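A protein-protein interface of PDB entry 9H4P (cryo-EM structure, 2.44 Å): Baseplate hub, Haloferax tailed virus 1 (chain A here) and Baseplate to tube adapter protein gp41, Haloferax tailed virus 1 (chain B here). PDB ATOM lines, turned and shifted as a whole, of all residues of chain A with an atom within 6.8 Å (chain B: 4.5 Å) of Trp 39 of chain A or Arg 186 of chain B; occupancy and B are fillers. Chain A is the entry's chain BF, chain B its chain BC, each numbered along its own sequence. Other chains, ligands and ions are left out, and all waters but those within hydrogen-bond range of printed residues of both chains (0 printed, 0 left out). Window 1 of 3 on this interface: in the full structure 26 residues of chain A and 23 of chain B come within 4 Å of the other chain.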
ATOM      1  N   ASN A  37      -5.385 -14.742  -6.917  1.00  0.00           N
ATOM      2  CA  ASN A  37      -4.096 -15.066  -7.564  1.00  0.00           C
ATOM      3  C   ASN A  37      -3.863 -16.572  -7.762  1.00  0.00           C
ATOM      4  O   ASN A  37      -2.727 -17.013  -7.924  1.00  0.00           O
ATOM      5  CB  ASN A  37      -2.954 -14.380  -6.812  1.00  0.00           C
ATOM      6  CG  ASN A  37      -3.175 -12.890  -6.674  1.00  0.00           C
ATOM      7  OD1 ASN A  37      -2.974 -12.116  -7.592  1.00  0.00           O
ATOM      8  ND2 ASN A  37      -3.583 -12.440  -5.517  1.00  0.00           N
ATOM      9  N   VAL A  38      -4.923 -17.373  -7.710  1.00  0.00           N
ATOM     10  CA  VAL A  38      -4.880 -18.836  -7.829  1.00  0.00           C
ATOM     11  C   VAL A  38      -4.512 -19.258  -9.243  1.00  0.00           C
ATOM     12  O   VAL A  38      -5.040 -18.711 -10.204  1.00  0.00           O
ATOM     13  CB  VAL A  38      -6.217 -19.463  -7.414  1.00  0.00           C
ATOM     14  CG1 VAL A  38      -6.143 -20.988  -7.355  1.00  0.00           C
ATOM     15  CG2 VAL A  38      -6.653 -18.987  -6.029  1.00  0.00           C
ATOM     16  N   TRP A  39      -3.625 -20.239  -9.380  1.00  0.00           N
ATOM     17  CA  TRP A  39      -3.164 -20.745 -10.674  1.00  0.00           C
ATOM     18  C   TRP A  39      -3.170 -22.266 -10.783  1.00  0.00           C
ATOM     19  O   TRP A  39      -2.983 -22.787 -11.881  1.00  0.00           O
ATOM     20  CB  TRP A  39      -1.792 -20.151 -10.997  1.00  0.00           C
ATOM     21  CG  TRP A  39      -0.694 -20.437 -10.025  1.00  0.00           C
ATOM     22  CD1 TRP A  39      -0.253 -19.581  -9.086  1.00  0.00           C
ATOM     23  CD2 TRP A  39       0.132 -21.629  -9.887  1.00  0.00           C
ATOM     24  NE1 TRP A  39       0.785 -20.154  -8.387  1.00  0.00           N
ATOM     25  CE2 TRP A  39       1.063 -21.415  -8.838  1.00  0.00           C
ATOM     26  CE3 TRP A  39       0.219 -22.861 -10.563  1.00  0.00           C
ATOM     27  CZ2 TRP A  39       2.003 -22.373  -8.454  1.00  0.00           C
ATOM     28  CZ3 TRP A  39       1.155 -23.836 -10.188  1.00  0.00           C
ATOM     29  CH2 TRP A  39       2.048 -23.597  -9.132  1.00  0.00           C
ATOM     30  N   ASP A  40      -3.430 -23.000  -9.704  1.00  0.00           N
ATOM     31  CA  ASP A  40      -3.815 -24.405  -9.793  1.00  0.00           C
ATOM     32  C   ASP A  40      -4.702 -24.843  -8.625  1.00  0.00           C
ATOM     33  O   ASP A  40      -4.595 -24.322  -7.520  1.00  0.00           O
ATOM     34  CB  ASP A  40      -2.570 -25.290  -9.891  1.00  0.00           C
ATOM     35  CG  ASP A  40      -2.844 -26.656 -10.520  1.00  0.00           C
ATOM     36  OD1 ASP A  40      -3.983 -26.897 -10.964  1.00  0.00           O
ATOM     37  OD2 ASP A  40      -1.908 -27.478 -10.566  1.00  0.00           O
ATOM     38  N   VAL A  41      -5.563 -25.822  -8.867  1.00  0.00           N
ATOM     39  CA  VAL A  41      -6.469 -26.426  -7.888  1.00  0.00           C
ATOM     40  C   VAL A  41      -6.480 -27.933  -8.101  1.00  0.00           C
ATOM     41  O   VAL A  41      -6.650 -28.398  -9.222  1.00  0.00           O
ATOM     42  CB  VAL A  41      -7.892 -25.854  -8.009  1.00  0.00           C
ATOM     43  CG1 VAL A  41      -8.908 -26.616  -7.160  1.00  0.00           C
ATOM     44  CG2 VAL A  41      -7.948 -24.387  -7.583  1.00  0.00           C
ATOM     45  N   PHE A  56      -4.620 -25.972  -3.124  1.00  0.00           N
ATOM     46  CA  PHE A  56      -4.694 -24.769  -3.946  1.00  0.00           C
ATOM     47  C   PHE A  56      -3.314 -24.152  -4.073  1.00  0.00           C
ATOM     48  O   PHE A  56      -2.617 -24.031  -3.074  1.00  0.00           O
ATOM     49  CB  PHE A  56      -5.650 -23.758  -3.318  1.00  0.00           C
ATOM     50  CG  PHE A  56      -6.953 -24.322  -2.816  1.00  0.00           C
ATOM     51  CD1 PHE A  56      -7.759 -25.108  -3.648  1.00  0.00           C
ATOM     52  CD2 PHE A  56      -7.363 -24.065  -1.504  1.00  0.00           C
ATOM     53  CE1 PHE A  56      -8.983 -25.613  -3.185  1.00  0.00           C
ATOM     54  CE2 PHE A  56      -8.577 -24.580  -1.035  1.00  0.00           C
ATOM     55  CZ  PHE A  56      -9.390 -25.351  -1.874  1.00  0.00           C
ATOM     56  N   LYS A  57      -2.920 -23.716  -5.264  1.00  0.00           N
ATOM     57  CA  LYS A  57      -1.661 -23.000  -5.478  1.00  0.00           C
ATOM     58  C   LYS A  57      -1.942 -21.608  -5.995  1.00  0.00           C
ATOM     59  O   LYS A  57      -2.740 -21.429  -6.911  1.00  0.00           O
ATOM     60  CB  LYS A  57      -0.755 -23.772  -6.432  1.00  0.00           C
ATOM     61  CG  LYS A  57      -0.340 -25.112  -5.831  1.00  0.00           C
ATOM     62  CD  LYS A  57       0.509 -25.906  -6.814  1.00  0.00           C
ATOM     63  CE  LYS A  57       0.799 -27.285  -6.228  1.00  0.00           C
ATOM     64  NZ  LYS A  57       1.419 -28.177  -7.233  1.00  0.00           N
ATOM     65  N   MET A  58      -1.292 -20.618  -5.415  1.00  0.00           N
ATOM     66  CA  MET A  58      -1.457 -19.215  -5.769  1.00  0.00           C
ATOM     67  C   MET A  58      -0.143 -18.468  -5.613  1.00  0.00           C
ATOM     68  O   MET A  58       0.749 -18.900  -4.893  1.00  0.00           O
ATOM     69  CB  MET A  58      -2.577 -18.606  -4.926  1.00  0.00           C
ATOM     70  CG  MET A  58      -2.268 -18.566  -3.438  1.00  0.00           C
ATOM     71  SD  MET A  58      -3.750 -18.677  -2.433  1.00  0.00           S
ATOM     72  CE  MET A  58      -4.063 -20.453  -2.497  1.00  0.00           C
ATOM     73  N   ASP A  59       0.008 -17.356  -6.310  1.00  0.00           N
ATOM     74  CA  ASP A  59       1.101 -16.432  -6.030  1.00  0.00           C
ATOM     75  C   ASP A  59       0.843 -15.630  -4.767  1.00  0.00           C
ATOM     76  O   ASP A  59      -0.301 -15.337  -4.432  1.00  0.00           O
ATOM     77  CB  ASP A  59       1.286 -15.467  -7.191  1.00  0.00           C
ATOM     78  CG  ASP A  59       2.038 -16.136  -8.320  1.00  0.00           C
ATOM     79  OD1 ASP A  59       3.265 -16.307  -8.181  1.00  0.00           O
ATOM     80  OD2 ASP A  59       1.400 -16.505  -9.332  1.00  0.00           O
ATOM     81  N   ASP A  60       1.911 -15.203  -4.106  1.00  0.00           N
ATOM     82  CA  ASP A  60       1.838 -14.297  -2.974  1.00  0.00           C
ATOM     83  C   ASP A  60       2.954 -13.240  -3.015  1.00  0.00           C
ATOM     84  O   ASP A  60       3.903 -13.338  -3.798  1.00  0.00           O
ATOM     85  CB  ASP A  60       1.798 -15.114  -1.678  1.00  0.00           C
ATOM     86  CG  ASP A  60       1.279 -14.308  -0.484  1.00  0.00           C
ATOM     87  OD1 ASP A  60       0.818 -13.164  -0.694  1.00  0.00           O
ATOM     88  OD2 ASP A  60       1.233 -14.829   0.646  1.00  0.00           O
ATOM     89  N   GLN A 102       9.953 -20.874  -5.370  1.00  0.00           N
ATOM     90  CA  GLN A 102       9.974 -21.838  -6.456  1.00  0.00           C
ATOM     91  C   GLN A 102      10.572 -21.178  -7.698  1.00  0.00           C
ATOM     92  O   GLN A 102       9.886 -20.482  -8.440  1.00  0.00           O
ATOM     93  CB  GLN A 102       8.542 -22.346  -6.618  1.00  0.00           C
ATOM     94  CG  GLN A 102       8.391 -23.423  -7.690  1.00  0.00           C
ATOM     95  CD  GLN A 102       6.923 -23.767  -7.900  1.00  0.00           C
ATOM     96  OE1 GLN A 102       6.266 -23.248  -8.788  1.00  0.00           O
ATOM     97  NE2 GLN A 102       6.355 -24.623  -7.084  1.00  0.00           N
ATOM     98  N   ASP A 106       7.304 -16.610  -5.408  1.00  0.00           N
ATOM     99  CA  ASP A 106       6.862 -16.915  -4.044  1.00  0.00           C
ATOM    100  C   ASP A 106       5.502 -17.600  -4.147  1.00  0.00           C
ATOM    101  O   ASP A 106       4.503 -16.937  -4.420  1.00  0.00           O
ATOM    102  CB  ASP A 106       6.762 -15.641  -3.193  1.00  0.00           C
ATOM    103  CG  ASP A 106       7.996 -14.749  -3.260  1.00  0.00           C
ATOM    104  OD1 ASP A 106       9.078 -15.157  -2.783  1.00  0.00           O
ATOM    105  OD2 ASP A 106       7.907 -13.654  -3.857  1.00  0.00           O
ATOM    106  N   VAL A 107       5.447 -18.921  -4.013  1.00  0.00           N
ATOM    107  CA  VAL A 107       4.197 -19.662  -4.197  1.00  0.00           C
ATOM    108  C   VAL A 107       3.618 -20.048  -2.858  1.00  0.00           C
ATOM    109  O   VAL A 107       4.311 -20.585  -2.006  1.00  0.00           O
ATOM    110  CB  VAL A 107       4.323 -20.880  -5.119  1.00  0.00           C
ATOM    111  CG1 VAL A 107       4.755 -20.452  -6.520  1.00  0.00           C
ATOM    112  CG2 VAL A 107       5.289 -21.954  -4.640  1.00  0.00           C
ATOM    113  N   LEU A 108       2.333 -19.789  -2.684  1.00  0.00           N
ATOM    114  CA  LEU A 108       1.557 -20.220  -1.542  1.00  0.00           C
ATOM    115  C   LEU A 108       0.768 -21.454  -1.954  1.00  0.00           C
ATOM    116  O   LEU A 108      -0.048 -21.410  -2.870  1.00  0.00           O
ATOM    117  CB  LEU A 108       0.664 -19.061  -1.105  1.00  0.00           C
ATOM    118  CG  LEU A 108      -0.426 -19.422  -0.092  1.00  0.00           C
ATOM    119  CD1 LEU A 108       0.139 -19.963   1.212  1.00  0.00           C
ATOM    120  CD2 LEU A 108      -1.208 -18.167   0.247  1.00  0.00           C
ATOM    121  N   TRP A 334      -7.354 -28.872 -12.007  1.00  0.00           N
ATOM    122  CA  TRP A 334      -7.310 -27.764 -12.953  1.00  0.00           C
ATOM    123  C   TRP A 334      -5.980 -27.825 -13.717  1.00  0.00           C
ATOM    124  O   TRP A 334      -5.243 -28.800 -13.585  1.00  0.00           O
ATOM    125  CB  TRP A 334      -7.497 -26.473 -12.172  1.00  0.00           C
ATOM    126  CG  TRP A 334      -7.992 -25.275 -12.912  1.00  0.00           C
ATOM    127  CD1 TRP A 334      -8.641 -25.251 -14.093  1.00  0.00           C
ATOM    128  CD2 TRP A 334      -8.027 -23.915 -12.414  1.00  0.00           C
ATOM    129  NE1 TRP A 334      -9.049 -23.965 -14.368  1.00  0.00           N
ATOM    130  CE2 TRP A 334      -8.730 -23.110 -13.346  1.00  0.00           C
ATOM    131  CE3 TRP A 334      -7.564 -23.297 -11.243  1.00  0.00           C
ATOM    132  CZ2 TRP A 334      -8.996 -21.763 -13.113  1.00  0.00           C
ATOM    133  CZ3 TRP A 334      -7.827 -21.945 -10.994  1.00  0.00           C
ATOM    134  CH2 TRP A 334      -8.559 -21.184 -11.914  1.00  0.00           C
ATOM    135  N   GLY A 335      -5.623 -26.839 -14.524  1.00  0.00           N
ATOM    136  CA  GLY A 335      -4.262 -26.712 -15.063  1.00  0.00           C
ATOM    137  C   GLY A 335      -3.940 -27.699 -16.185  1.00  0.00           C
ATOM    138  O   GLY A 335      -3.830 -27.295 -17.336  1.00  0.00           O
ATOM    139  N   VAL A 336      -3.834 -28.994 -15.878  1.00  0.00           N
ATOM    140  CA  VAL A 336      -3.869 -30.100 -16.855  1.00  0.00           C
ATOM    141  C   VAL A 336      -5.296 -30.481 -17.251  1.00  0.00           C
ATOM    142  O   VAL A 336      -5.499 -31.204 -18.222  1.00  0.00           O
ATOM    143  CB  VAL A 336      -3.124 -31.341 -16.343  1.00  0.00           C
ATOM    144  CG1 VAL A 336      -1.656 -31.034 -16.074  1.00  0.00           C
ATOM    145  CG2 VAL A 336      -3.720 -31.926 -15.069  1.00  0.00           C
ATOM    146  N   GLU B  34      -0.807 -22.893 -22.746  1.00  0.00           N
ATOM    147  CA  GLU B  34      -1.665 -23.498 -21.733  1.00  0.00           C
ATOM    148  C   GLU B  34      -2.875 -24.227 -22.335  1.00  0.00           C
ATOM    149  O   GLU B  34      -3.817 -24.525 -21.594  1.00  0.00           O
ATOM    150  CB  GLU B  34      -2.101 -22.457 -20.688  1.00  0.00           C
ATOM    151  CG  GLU B  34      -0.957 -21.783 -19.941  1.00  0.00           C
ATOM    152  CD  GLU B  34      -0.023 -22.704 -19.178  1.00  0.00           C
ATOM    153  OE1 GLU B  34      -0.519 -23.589 -18.462  1.00  0.00           O
ATOM    154  OE2 GLU B  34       1.202 -22.539 -19.311  1.00  0.00           O
ATOM    155  N   TRP B  52      -7.180 -20.491 -20.586  1.00  0.00           N
ATOM    156  CA  TRP B  52      -6.242 -19.614 -19.896  1.00  0.00           C
ATOM    157  C   TRP B  52      -5.825 -18.474 -20.828  1.00  0.00           C
ATOM    158  O   TRP B  52      -6.123 -18.509 -22.025  1.00  0.00           O
ATOM    159  CB  TRP B  52      -5.019 -20.423 -19.425  1.00  0.00           C
ATOM    160  CG  TRP B  52      -5.305 -21.525 -18.444  1.00  0.00           C
ATOM    161  CD1 TRP B  52      -5.546 -22.841 -18.726  1.00  0.00           C
ATOM    162  CD2 TRP B  52      -5.363 -21.412 -17.005  1.00  0.00           C
ATOM    163  NE1 TRP B  52      -5.754 -23.545 -17.566  1.00  0.00           N
ATOM    164  CE2 TRP B  52      -5.651 -22.697 -16.489  1.00  0.00           C
ATOM    165  CE3 TRP B  52      -5.207 -20.352 -16.097  1.00  0.00           C
ATOM    166  CZ2 TRP B  52      -5.774 -22.937 -15.112  1.00  0.00           C
ATOM    167  CZ3 TRP B  52      -5.323 -20.588 -14.740  1.00  0.00           C
ATOM    168  CH2 TRP B  52      -5.606 -21.867 -14.253  1.00  0.00           C
ATOM    169  N   SER B  53      -5.124 -17.478 -20.262  1.00  0.00           N
ATOM    170  CA  SER B  53      -4.487 -16.409 -21.022  1.00  0.00           C
ATOM    171  C   SER B  53      -3.504 -16.976 -22.050  1.00  0.00           C
ATOM    172  O   SER B  53      -2.866 -18.005 -21.808  1.00  0.00           O
ATOM    173  CB  SER B  53      -3.807 -15.425 -20.091  1.00  0.00           C
ATOM    174  OG  SER B  53      -2.947 -16.087 -19.169  1.00  0.00           O
ATOM    175  N   VAL B 184       5.754 -14.486 -14.707  1.00  0.00           N
ATOM    176  CA  VAL B 184       4.621 -14.207 -15.581  1.00  0.00           C
ATOM    177  C   VAL B 184       3.723 -15.448 -15.555  1.00  0.00           C
ATOM    178  O   VAL B 184       4.176 -16.542 -15.895  1.00  0.00           O
ATOM    179  CB  VAL B 184       5.089 -13.834 -17.009  1.00  0.00           C
ATOM    180  CG1 VAL B 184       3.936 -13.625 -17.978  1.00  0.00           C
ATOM    181  CG2 VAL B 184       6.004 -12.612 -17.022  1.00  0.00           C
ATOM    182  N   ARG B 185       2.458 -15.268 -15.142  1.00  0.00           N
ATOM    183  CA  ARG B 185       1.599 -16.381 -14.760  1.00  0.00           C
ATOM    184  C   ARG B 185       0.293 -16.377 -15.552  1.00  0.00           C
ATOM    185  O   ARG B 185      -0.297 -15.322 -15.786  1.00  0.00           O
ATOM    186  CB  ARG B 185       1.322 -16.328 -13.252  1.00  0.00           C
ATOM    187  CG  ARG B 185       2.299 -17.158 -12.434  1.00  0.00           C
ATOM    188  CD  ARG B 185       1.741 -18.537 -12.113  1.00  0.00           C
ATOM    189  NE  ARG B 185       2.744 -19.491 -11.650  1.00  0.00           N
ATOM    190  CZ  ARG B 185       3.478 -19.380 -10.540  1.00  0.00           C
ATOM    191  NH1 ARG B 185       4.349 -20.324 -10.231  1.00  0.00           N
ATOM    192  NH2 ARG B 185       3.359 -18.330  -9.746  1.00  0.00           N
ATOM    193  N   ARG B 186      -0.161 -17.589 -15.913  1.00  0.00           N
ATOM    194  CA  ARG B 186      -1.467 -17.832 -16.514  1.00  0.00           C
ATOM    195  C   ARG B 186      -2.593 -17.342 -15.597  1.00  0.00           C
ATOM    196  O   ARG B 186      -2.508 -17.454 -14.369  1.00  0.00           O
ATOM    197  CB  ARG B 186      -1.637 -19.318 -16.867  1.00  0.00           C
ATOM    198  CG  ARG B 186      -1.731 -20.272 -15.679  1.00  0.00           C
ATOM    199  CD  ARG B 186      -1.859 -21.718 -16.124  1.00  0.00           C
ATOM    200  NE  ARG B 186      -1.978 -22.584 -14.957  1.00  0.00           N
ATOM    201  CZ  ARG B 186      -1.499 -23.823 -14.844  1.00  0.00           C
ATOM    202  NH1 ARG B 186      -1.678 -24.490 -13.715  1.00  0.00           N
ATOM    203  NH2 ARG B 186      -0.840 -24.397 -15.839  1.00  0.00           N
ATOM    204  N   VAL B 187      -3.648 -16.798 -16.225  1.00  0.00           N
ATOM    205  CA  VAL B 187      -4.871 -16.394 -15.542  1.00  0.00           C
ATOM    206  C   VAL B 187      -6.071 -16.974 -16.295  1.00  0.00           C
ATOM    207  O   VAL B 187      -6.016 -17.109 -17.520  1.00  0.00           O
ATOM    208  CB  VAL B 187      -4.984 -14.861 -15.387  1.00  0.00           C
ATOM    209  CG1 VAL B 187      -4.041 -14.314 -14.322  1.00  0.00           C
ATOM    210  CG2 VAL B 187      -4.815 -14.113 -16.706  1.00  0.00           C
ATOM    211  N   ARG B 194      -0.746 -12.449 -15.822  1.00  0.00           N
ATOM    212  CA  ARG B 194      -0.452 -11.624 -14.659  1.00  0.00           C
ATOM    213  C   ARG B 194       1.068 -11.565 -14.461  1.00  0.00           C
ATOM    214  O   ARG B 194       1.768 -12.549 -14.710  1.00  0.00           O
ATOM    215  CB  ARG B 194      -1.244 -12.191 -13.472  1.00  0.00           C
ATOM    216  CG  ARG B 194      -0.917 -11.603 -12.107  1.00  0.00           C
ATOM    217  CD  ARG B 194      -1.829 -12.095 -10.999  1.00  0.00           C
ATOM    218  NE  ARG B 194      -2.153 -13.523 -11.045  1.00  0.00           N
ATOM    219  CZ  ARG B 194      -1.375 -14.536 -10.648  1.00  0.00           C
ATOM    220  NH1 ARG B 194      -1.818 -15.779 -10.751  1.00  0.00           N
ATOM    221  NH2 ARG B 194      -0.169 -14.319 -10.152  1.00  0.00           N
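The backbone carbonyl oxygen (O) of Trp 39 of chain A sits at hydrogen-bond distance from the guanidinium group (NH1) of Arg 186 of chain B, 2.8 Å away. OD1 of Asp 59 of chain A lies within salt-bridge range of NH2 of Arg 185 of chain B. The guanidinium group (NH2) of Arg 194 of chain B lies within salt-bridge range of the side-chain carboxylate (OD2) of Asp 59 of chain A (2.8 Å). The indole nitrogen (NE1) of Trp 39 of chain A lies close to the guanidinium group (NH2) of Arg 185 of chain B (3.4 Å). The backbone carbonyl oxygen of Asn 37 of chain A is in hydrogen-bond range of the guanidinium group of Arg 194 of chain B (3.2 Å).
Trp 39 of chain A touches just these residues of chain B: Trp 52 (3.7 Å), Arg 185 (3.4 Å) and Arg 186 (2.8 Å). Of the printed residues of chain A, Arg 186 of chain B touches Trp 39 (2.8 Å) and Gly 335 (3.7 Å). Of the printed residues of chain B, Asp 59 of chain A touches Arg 185 (2.6 Å) and Arg 194 (2.8 Å). Of the printed residues of chain A, Arg 194 of chain B touches Asn 37 (3.2 Å) and Asp 59 (2.8 Å). Of the printed residues of chain A, Arg 185 of chain B touches Trp 39 (3.4 Å), Asp 59 (2.6 Å), Gln 102 (3.8 Å) and Val 107 (3.7 Å). Val 336 of chain A touches none of the printed residues of chain B. The nearest residue of chain B that does not touch Trp 39 of chain A is Arg 194 of chain B (4.4 Å). The nearest printed residue of chain A that does not touch Arg 186 of chain B is Asp 40 of chain A (4.01 Å).
OE1 of Glu 34 of chain B lies within salt-bridge range of NH2 of Arg 186 of chain B (2.8 Å). The backbone NH (N) of Trp 334 of chain A lies within hydrogen-bond range of the backbone carbonyl oxygen (O) of Val 41 of chain A (2.9 Å). The backbone NH (N) of Arg 185 of chain B is in hydrogen-bond range of the backbone carbonyl oxygen (O) of Arg 194 of chain B (2.8 Å). The backbone carbonyl oxygen of Asn 37 of chain A is in hydrogen-bond range of the backbone NH of Asp 59 of chain A (3.2 Å). N of Trp 39 of chain A is in hydrogen-bond range of O of Lys 57 of chain A.
Trp 39 of chain A touches Trp 52 of chain B (O to CH2, 3.7 Å). Gln 102 of chain A touches Arg 185 of chain B (OE1 to NH1, 3.8 Å). Val 107 of chain A touches Arg 185 of chain B (CG1 to NH1, 3.7 Å). Trp 334 of chain A touches Trp 52 of chain B. Gly 335 of chain A touches Trp 52 of chain B (N to CZ2, 3.9 Å). NH1 of Arg 186 of chain B touches CA of Gly 335 of chain A (3.7 Å).
Hydrophobic or aromatic side chains of chain B that line the printed part of chain A: Trp 52. Printed residues of chain A that touch a printed residue of chain B: Asn 37, Trp 39, Asp 59, Gln 102, Val 107, Trp 334 and Gly 335. Hydrophobic or aromatic side chains of chain A that line the printed part of chain B: Trp 39, Val 107 and Trp 334. Among the printed residues, Asp or Glu carboxylates within 4 Å of a Lys or Arg side-chain nitrogen of the other chain: Asp 59 of chain A with Arg 185 of chain B and Asp 59 of chain A with Arg 194 of chain B.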
